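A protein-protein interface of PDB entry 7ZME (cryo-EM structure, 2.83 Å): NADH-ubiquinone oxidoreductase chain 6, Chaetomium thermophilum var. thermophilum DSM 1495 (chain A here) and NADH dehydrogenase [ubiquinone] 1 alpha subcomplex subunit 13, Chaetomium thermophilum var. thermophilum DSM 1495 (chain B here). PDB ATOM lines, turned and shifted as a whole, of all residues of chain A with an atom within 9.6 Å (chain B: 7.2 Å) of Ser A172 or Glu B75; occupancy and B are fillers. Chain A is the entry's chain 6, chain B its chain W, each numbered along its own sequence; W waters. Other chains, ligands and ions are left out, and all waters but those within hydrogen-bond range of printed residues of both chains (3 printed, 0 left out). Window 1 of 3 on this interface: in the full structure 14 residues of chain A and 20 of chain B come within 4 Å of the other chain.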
ATOM      1  N   PHE A 169      -6.268  39.726   9.408  1.00  0.00           N
ATOM      2  CA  PHE A 169      -6.212  38.313   9.841  1.00  0.00           C
ATOM      3  C   PHE A 169      -5.457  37.496   8.802  1.00  0.00           C
ATOM      4  O   PHE A 169      -5.677  37.687   7.607  1.00  0.00           O
ATOM      5  CB  PHE A 169      -7.622  37.803  10.124  1.00  0.00           C
ATOM      6  CG  PHE A 169      -8.313  38.483  11.276  1.00  0.00           C
ATOM      7  CD1 PHE A 169      -7.958  38.194  12.581  1.00  0.00           C
ATOM      8  CD2 PHE A 169      -9.316  39.407  11.054  1.00  0.00           C
ATOM      9  CE1 PHE A 169      -8.598  38.818  13.639  1.00  0.00           C
ATOM     10  CE2 PHE A 169      -9.952  40.032  12.114  1.00  0.00           C
ATOM     11  CZ  PHE A 169      -9.590  39.737  13.405  1.00  0.00           C
ATOM     12  N   ILE A 170      -4.593  36.603   9.267  1.00  0.00           N
ATOM     13  CA  ILE A 170      -3.751  35.779   8.352  1.00  0.00           C
ATOM     14  C   ILE A 170      -4.086  34.300   8.568  1.00  0.00           C
ATOM     15  O   ILE A 170      -4.169  33.880   9.728  1.00  0.00           O
ATOM     16  CB  ILE A 170      -2.256  36.122   8.519  1.00  0.00           C
ATOM     17  CG1 ILE A 170      -1.414  35.604   7.352  1.00  0.00           C
ATOM     18  CG2 ILE A 170      -1.706  35.683   9.863  1.00  0.00           C
ATOM     19  CD1 ILE A 170      -1.493  36.462   6.120  1.00  0.00           C
ATOM     20  N   THR A 171      -4.344  33.564   7.489  1.00  0.00           N
ATOM     21  CA  THR A 171      -4.613  32.137   7.588  1.00  0.00           C
ATOM     22  C   THR A 171      -3.711  31.370   6.634  1.00  0.00           C
ATOM     23  O   THR A 171      -3.386  31.838   5.542  1.00  0.00           O
ATOM     24  CB  THR A 171      -6.079  31.783   7.283  1.00  0.00           C
ATOM     25  OG1 THR A 171      -6.334  31.938   5.883  1.00  0.00           O
ATOM     26  CG2 THR A 171      -7.029  32.660   8.073  1.00  0.00           C
ATOM     27  N   SER A 172      -3.322  30.156   7.034  1.00  0.00           N
ATOM     28  CA  SER A 172      -2.484  29.273   6.182  1.00  0.00           C
ATOM     29  C   SER A 172      -3.145  27.896   6.131  1.00  0.00           C
ATOM     30  O   SER A 172      -4.301  27.796   6.556  1.00  0.00           O
ATOM     31  CB  SER A 172      -1.078  29.188   6.683  1.00  0.00           C
ATOM     32  OG  SER A 172      -1.014  28.437   7.878  1.00  0.00           O
ATOM     33  N   LYS A 173      -2.426  26.869   5.674  1.00  0.00           N
ATOM     34  CA  LYS A 173      -3.058  25.538   5.486  1.00  0.00           C
ATOM     35  C   LYS A 173      -2.412  24.447   6.353  1.00  0.00           C
ATOM     36  O   LYS A 173      -1.254  24.631   6.738  1.00  0.00           O
ATOM     37  CB  LYS A 173      -2.975  25.211   3.996  1.00  0.00           C
ATOM     38  CG  LYS A 173      -1.615  24.791   3.463  1.00  0.00           C
ATOM     39  CD  LYS A 173      -1.652  24.439   1.997  1.00  0.00           C
ATOM     40  CE  LYS A 173      -2.226  25.544   1.136  1.00  0.00           C
ATOM     41  NZ  LYS A 173      -2.268  25.155  -0.291  1.00  0.00           N
ATOM     42  N   ILE A 174      -3.152  23.383   6.697  1.00  0.00           N
ATOM     43  CA  ILE A 174      -2.546  22.204   7.402  1.00  0.00           C
ATOM     44  C   ILE A 174      -2.980  20.932   6.684  1.00  0.00           C
ATOM     45  O   ILE A 174      -4.027  20.945   6.039  1.00  0.00           O
ATOM     46  CB  ILE A 174      -2.830  22.087   8.917  1.00  0.00           C
ATOM     47  CG1 ILE A 174      -4.318  22.190   9.258  1.00  0.00           C
ATOM     48  CG2 ILE A 174      -1.973  23.049   9.726  1.00  0.00           C
ATOM     49  CD1 ILE A 174      -4.636  21.759  10.669  1.00  0.00           C
ATOM     50  N   TRP A 175      -2.168  19.889   6.783  1.00  0.00           N
ATOM     51  CA  TRP A 175      -2.462  18.620   6.081  1.00  0.00           C
ATOM     52  C   TRP A 175      -2.962  17.542   7.047  1.00  0.00           C
ATOM     53  O   TRP A 175      -3.871  16.802   6.662  1.00  0.00           O
ATOM     54  CB  TRP A 175      -1.212  18.216   5.297  1.00  0.00           C
ATOM     55  CG  TRP A 175      -0.893  19.219   4.234  1.00  0.00           C
ATOM     56  CD1 TRP A 175       0.063  20.189   4.280  1.00  0.00           C
ATOM     57  CD2 TRP A 175      -1.577  19.390   2.981  1.00  0.00           C
ATOM     58  NE1 TRP A 175       0.043  20.929   3.131  1.00  0.00           N
ATOM     59  CE2 TRP A 175      -0.955  20.466   2.316  1.00  0.00           C
ATOM     60  CE3 TRP A 175      -2.639  18.734   2.350  1.00  0.00           C
ATOM     61  CZ2 TRP A 175      -1.361  20.896   1.055  1.00  0.00           C
ATOM     62  CZ3 TRP A 175      -3.041  19.160   1.105  1.00  0.00           C
ATOM     63  CH2 TRP A 175      -2.406  20.224   0.469  1.00  0.00           C
ATOM     64  N   ASP A 176      -2.392  17.470   8.248  1.00  0.00           N
ATOM     65  CA  ASP A 176      -2.811  16.482   9.279  1.00  0.00           C
ATOM     66  C   ASP A 176      -4.245  16.754   9.756  1.00  0.00           C
ATOM     67  O   ASP A 176      -4.991  15.786   9.963  1.00  0.00           O
ATOM     68  CB  ASP A 176      -1.760  16.343  10.383  1.00  0.00           C
ATOM     69  CG  ASP A 176      -1.110  17.652  10.800  1.00  0.00           C
ATOM     70  OD1 ASP A 176      -0.075  17.592  11.492  1.00  0.00           O
ATOM     71  OD2 ASP A 176      -1.647  18.720  10.451  1.00  0.00           O
ATOM     72  N   ALA A 178      -6.481  18.304   7.996  1.00  0.00           N
ATOM     73  CA  ALA A 178      -7.382  18.300   6.823  1.00  0.00           C
ATOM     74  C   ALA A 178      -7.560  16.896   6.249  1.00  0.00           C
ATOM     75  O   ALA A 178      -8.014  16.815   5.100  1.00  0.00           O
ATOM     76  CB  ALA A 178      -6.868  19.240   5.768  1.00  0.00           C
ATOM     77  N   LEU B  70       4.906  14.316   3.794  1.00  0.00           N
ATOM     78  CA  LEU B  70       5.701  15.195   2.895  1.00  0.00           C
ATOM     79  C   LEU B  70       5.057  16.571   2.714  1.00  0.00           C
ATOM     80  O   LEU B  70       5.800  17.556   2.618  1.00  0.00           O
ATOM     81  CB  LEU B  70       5.964  14.482   1.562  1.00  0.00           C
ATOM     82  CG  LEU B  70       4.753  14.101   0.711  1.00  0.00           C
ATOM     83  CD1 LEU B  70       4.546  15.094  -0.424  1.00  0.00           C
ATOM     84  CD2 LEU B  70       4.931  12.705   0.139  1.00  0.00           C
ATOM     85  N   LEU B  71       3.733  16.637   2.721  1.00  0.00           N
ATOM     86  CA  LEU B  71       3.007  17.922   2.565  1.00  0.00           C
ATOM     87  C   LEU B  71       3.181  18.767   3.827  1.00  0.00           C
ATOM     88  O   LEU B  71       3.495  19.948   3.691  1.00  0.00           O
ATOM     89  CB  LEU B  71       1.546  17.635   2.215  1.00  0.00           C
ATOM     90  CG  LEU B  71       1.294  17.120   0.800  1.00  0.00           C
ATOM     91  CD1 LEU B  71      -0.082  16.489   0.699  1.00  0.00           C
ATOM     92  CD2 LEU B  71       1.450  18.233  -0.218  1.00  0.00           C
ATOM     93  N   GLN B  72       2.951  18.185   5.000  1.00  0.00           N
ATOM     94  CA  GLN B  72       3.090  18.896   6.296  1.00  0.00           C
ATOM     95  C   GLN B  72       4.539  19.335   6.500  1.00  0.00           C
ATOM     96  O   GLN B  72       4.740  20.379   7.117  1.00  0.00           O
ATOM     97  CB  GLN B  72       2.572  18.020   7.436  1.00  0.00           C
ATOM     98  CG  GLN B  72       2.440  18.743   8.766  1.00  0.00           C
ATOM     99  CD  GLN B  72       1.490  19.914   8.732  1.00  0.00           C
ATOM    100  OE1 GLN B  72       0.539  19.951   7.959  1.00  0.00           O
ATOM    101  NE2 GLN B  72       1.736  20.884   9.596  1.00  0.00           N
ATOM    102  N   ALA B  73       5.508  18.596   5.967  1.00  0.00           N
ATOM    103  CA  ALA B  73       6.936  18.931   6.170  1.00  0.00           C
ATOM    104  C   ALA B  73       7.260  20.202   5.385  1.00  0.00           C
ATOM    105  O   ALA B  73       7.940  21.068   5.945  1.00  0.00           O
ATOM    106  CB  ALA B  73       7.770  17.783   5.682  1.00  0.00           C
ATOM    107  N   GLU B  74       6.767  20.318   4.156  1.00  0.00           N
ATOM    108  CA  GLU B  74       6.929  21.535   3.334  1.00  0.00           C
ATOM    109  C   GLU B  74       6.224  22.707   4.004  1.00  0.00           C
ATOM    110  O   GLU B  74       6.768  23.820   3.946  1.00  0.00           O
ATOM    111  CB  GLU B  74       6.235  21.273   2.007  1.00  0.00           C
ATOM    112  CG  GLU B  74       6.297  22.431   1.033  1.00  0.00           C
ATOM    113  CD  GLU B  74       5.180  22.414   0.009  1.00  0.00           C
ATOM    114  OE1 GLU B  74       4.563  21.349  -0.176  1.00  0.00           O
ATOM    115  OE2 GLU B  74       4.917  23.470  -0.583  1.00  0.00           O
ATOM    116  N   GLU B  75       5.035  22.475   4.566  1.00  0.00           N
ATOM    117  CA  GLU B  75       4.252  23.537   5.252  1.00  0.00           C
ATOM    118  C   GLU B  75       4.998  24.026   6.493  1.00  0.00           C
ATOM    119  O   GLU B  75       5.002  25.232   6.738  1.00  0.00           O
ATOM    120  CB  GLU B  75       2.840  23.035   5.561  1.00  0.00           C
ATOM    121  CG  GLU B  75       1.912  24.111   6.090  1.00  0.00           C
ATOM    122  CD  GLU B  75       1.543  25.219   5.117  1.00  0.00           C
ATOM    123  OE1 GLU B  75       1.704  25.022   3.899  1.00  0.00           O
ATOM    124  OE2 GLU B  75       1.084  26.277   5.582  1.00  0.00           O
ATOM    125  N   ASP B  76       5.615  23.110   7.231  1.00  0.00           N
ATOM    126  CA  ASP B  76       6.352  23.467   8.469  1.00  0.00           C
ATOM    127  C   ASP B  76       7.604  24.257   8.117  1.00  0.00           C
ATOM    128  O   ASP B  76       7.925  25.181   8.859  1.00  0.00           O
ATOM    129  CB  ASP B  76       6.780  22.226   9.243  1.00  0.00           C
ATOM    130  CG  ASP B  76       5.652  21.514   9.956  1.00  0.00           C
ATOM    131  OD1 ASP B  76       4.482  21.833   9.681  1.00  0.00           O
ATOM    132  OD2 ASP B  76       5.961  20.655  10.788  1.00  0.00           O
ATOM    133  N   ARG B  77       8.277  23.892   7.025  1.00  0.00           N
ATOM    134  CA  ARG B  77       9.481  24.648   6.599  1.00  0.00           C
ATOM    135  C   ARG B  77       9.075  26.085   6.279  1.00  0.00           C
ATOM    136  O   ARG B  77       9.841  26.985   6.625  1.00  0.00           O
ATOM    137  CB  ARG B  77      10.175  23.939   5.433  1.00  0.00           C
ATOM    138  CG  ARG B  77      11.044  22.763   5.843  1.00  0.00           C
ATOM    139  CD  ARG B  77      11.816  22.257   4.646  1.00  0.00           C
ATOM    140  NE  ARG B  77      10.976  21.593   3.664  1.00  0.00           N
ATOM    141  CZ  ARG B  77      10.802  20.281   3.592  1.00  0.00           C
ATOM    142  NH1 ARG B  77      11.417  19.484   4.447  1.00  0.00           N
ATOM    143  NH2 ARG B  77      10.017  19.772   2.662  1.00  0.00           N
ATOM    144  N   ASP B  78       7.917  26.276   5.652  1.00  0.00           N
ATOM    145  CA  ASP B  78       7.394  27.627   5.326  1.00  0.00           C
ATOM    146  C   ASP B  78       7.062  28.386   6.615  1.00  0.00           C
ATOM    147  O   ASP B  78       7.326  29.585   6.660  1.00  0.00           O
ATOM    148  CB  ASP B  78       6.150  27.500   4.445  1.00  0.00           C
ATOM    149  CG  ASP B  78       5.797  28.773   3.697  1.00  0.00           C
ATOM    150  OD1 ASP B  78       6.340  28.971   2.595  1.00  0.00           O
ATOM    151  OD2 ASP B  78       4.976  29.553   4.216  1.00  0.00           O
ATOM    152  N   HIS B  79       6.497  27.704   7.607  1.00  0.00           N
ATOM    153  CA  HIS B  79       6.098  28.353   8.875  1.00  0.00           C
ATOM    154  C   HIS B  79       7.323  28.783   9.661  1.00  0.00           C
ATOM    155  O   HIS B  79       7.287  29.893  10.198  1.00  0.00           O
ATOM    156  CB  HIS B  79       5.190  27.411   9.674  1.00  0.00           C
ATOM    157  CG  HIS B  79       3.758  27.515   9.278  1.00  0.00           C
ATOM    158  ND1 HIS B  79       2.825  28.151  10.061  1.00  0.00           N
ATOM    159  CD2 HIS B  79       3.108  27.097   8.173  1.00  0.00           C
ATOM    160  CE1 HIS B  79       1.654  28.100   9.468  1.00  0.00           C
ATOM    161  NE2 HIS B  79       1.801  27.460   8.310  1.00  0.00           N
ATOM    162  N   VAL B  80       8.334  27.918   9.735  1.00  0.00           N
ATOM    163  CA  VAL B  80       9.583  28.224  10.471  1.00  0.00           C
ATOM    164  C   VAL B  80      10.233  29.390   9.746  1.00  0.00           C
ATOM    165  O   VAL B  80      10.612  30.333  10.420  1.00  0.00           O
ATOM    166  CB  VAL B  80      10.481  26.968  10.554  1.00  0.00           C
ATOM    167  CG1 VAL B  80      11.905  27.270  10.993  1.00  0.00           C
ATOM    168  CG2 VAL B  80       9.866  25.872  11.406  1.00  0.00           C
ATOM    169  N   ARG B  81      10.220  29.378   8.413  1.00  0.00           N
ATOM    170  CA  ARG B  81      10.892  30.438   7.622  1.00  0.00           C
ATOM    171  C   ARG B  81      10.195  31.788   7.835  1.00  0.00           C
ATOM    172  O   ARG B  81      10.907  32.782   8.011  1.00  0.00           O
ATOM    173  CB  ARG B  81      10.817  30.045   6.148  1.00  0.00           C
ATOM    174  CG  ARG B  81      11.423  31.043   5.176  1.00  0.00           C
ATOM    175  CD  ARG B  81      11.212  30.618   3.735  1.00  0.00           C
ATOM    176  NE  ARG B  81       9.807  30.568   3.358  1.00  0.00           N
ATOM    177  CZ  ARG B  81       9.119  31.594   2.874  1.00  0.00           C
ATOM    178  NH1 ARG B  81       7.845  31.450   2.562  1.00  0.00           N
ATOM    179  NH2 ARG B  81       9.705  32.764   2.710  1.00  0.00           N
ATOM    180  N   TYR B 106       5.333  27.059  19.401  1.00  0.00           N
ATOM    181  CA  TYR B 106       4.982  27.846  18.200  1.00  0.00           C
ATOM    182  C   TYR B 106       3.471  28.030  18.146  1.00  0.00           C
ATOM    183  O   TYR B 106       2.748  27.041  18.326  1.00  0.00           O
ATOM    184  CB  TYR B 106       5.404  27.139  16.911  1.00  0.00           C
ATOM    185  CG  TYR B 106       4.969  27.861  15.664  1.00  0.00           C
ATOM    186  CD1 TYR B 106       5.357  29.169  15.437  1.00  0.00           C
ATOM    187  CD2 TYR B 106       4.154  27.251  14.725  1.00  0.00           C
ATOM    188  CE1 TYR B 106       4.956  29.854  14.305  1.00  0.00           C
ATOM    189  CE2 TYR B 106       3.745  27.924  13.586  1.00  0.00           C
ATOM    190  CZ  TYR B 106       4.150  29.229  13.375  1.00  0.00           C
ATOM    191  OH  TYR B 106       3.766  29.915  12.263  1.00  0.00           O
ATOM    192  N   ARG B 108       0.551  29.373  15.464  1.00  0.00           N
ATOM    193  CA  ARG B 108       0.281  29.926  14.115  1.00  0.00           C
ATOM    194  C   ARG B 108      -0.311  31.333  14.239  1.00  0.00           C
ATOM    195  O   ARG B 108      -1.313  31.496  14.952  1.00  0.00           O
ATOM    196  CB  ARG B 108      -0.637  28.974  13.344  1.00  0.00           C
ATOM    197  CG  ARG B 108       0.090  27.776  12.756  1.00  0.00           C
ATOM    198  CD  ARG B 108      -0.787  26.547  12.665  1.00  0.00           C
ATOM    199  NE  ARG B 108      -0.058  25.382  12.186  1.00  0.00           N
ATOM    200  CZ  ARG B 108       0.523  24.479  12.968  1.00  0.00           C
ATOM    201  NH1 ARG B 108       1.155  23.450  12.433  1.00  0.00           N
ATOM    202  NH2 ARG B 108       0.467  24.603  14.280  1.00  0.00           N
ATOM    203  N   PRO B 109       0.252  32.342  13.534  1.00  0.00           N
ATOM    204  CA  PRO B 109      -0.199  33.733  13.666  1.00  0.00           C
ATOM    205  C   PRO B 109      -1.653  34.037  13.284  1.00  0.00           C
ATOM    206  O   PRO B 109      -2.076  33.602  12.256  1.00  0.00           O
ATOM    207  CB  PRO B 109       0.683  34.437  12.626  1.00  0.00           C
ATOM    208  CG  PRO B 109       1.921  33.596  12.521  1.00  0.00           C
ATOM    209  CD  PRO B 109       1.394  32.187  12.635  1.00  0.00           C
HETATM  210  O   HOH W   1       1.739  22.903   1.146  1.00  0.00           O
HETATM  211  O   HOH W   2      -1.613  26.356   9.496  1.00  0.00           O
HETATM  212  O   HOH W   3      -0.266  28.348   3.472  1.00  0.00           O
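Among the printed residues, pairs that only touch across the chains: Ser A172 with Glu B75 (3.8 Å), Ile A174 with Gln B72 (3.9 Å), Ile A174 with Arg B108 (3.9 Å), Trp A175 with Leu B71 (3.5 Å) and Asp A176 with Gln B72 (3.5 Å).
The side-chain amide oxygen (OE1) of Gln B72 sits at hydrogen-bond distance from the backbone NH (N) of Trp A175.
OG of Ser A172 is in hydrogen-bond range of NE2 of His B79 (3.0 Å).
The backbone carbonyl oxygen (O) of Ile A170 sits close to the backbone carbonyl oxygen (O) of Pro B109 (3.3 Å).
The side-chain carboxylate (OE2) of Glu B75 sits close to the backbone carbonyl oxygen (O) of Lys A173 (3.1 Å).
Of the 9 printed residues of chain A, 6 touch a printed residue of chain B.
Hydrophobic or aromatic side chains of chain A within 4 Å of the printed part of chain B: Ile A170, Ile A174 and Trp A175.
Of chain B, only Glu B75 and His B79 come within 4 Å of Ser A172.
Glu B75 touches just these residues of chain A: Ser A172 and Lys A173.
Of chain A, only Ile A174, Trp A175 and Asp A176 come within 4 Å of Gln B72.
No residue of chain A comes within 4 Å of Glu B74.
Of the printed residues of chain A, Leu B71 touches Trp A175 (3.5 Å).
Of the printed residues of chain B, Lys A173 touches Glu B75.
Printed residues of chain A within 4 Å of His B79: Ser A172.
The nearest residue of chain B that does not touch Ser A172 is Arg B108 (5.0 Å).
The nearest printed residue of chain B that does not touch Trp A175 is Glu B75 (4.2 Å).
Water W2 lies within hydrogen-bond range of the side-chain hydroxyl of Ser A172 (2.7 Å), the guanidinium group of Arg B108 (3.3 Å) and the backbone carbonyl oxygen of Lys A173 (3.3 Å).
Water W3 lies within hydrogen-bond range of OE2 of Glu B75 and N of Lys A173.
Water W1 lies within hydrogen-bond range of NE1 of Trp A175, OE1 of Glu B75 and OE1 of Glu B74.
The side-chain carboxylate of Asp B76 lies within hydrogen-bond range of the side-chain amide nitrogen of Gln B72.
The side-chain carboxylate (OE2) of Glu B75 lies within hydrogen-bond range of a ring nitrogen (NE2) of His B79 (3.1 Å).
A ring nitrogen (ND1) of His B79 lies within hydrogen-bond range of the side-chain hydroxyl (OH) of Tyr B106.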
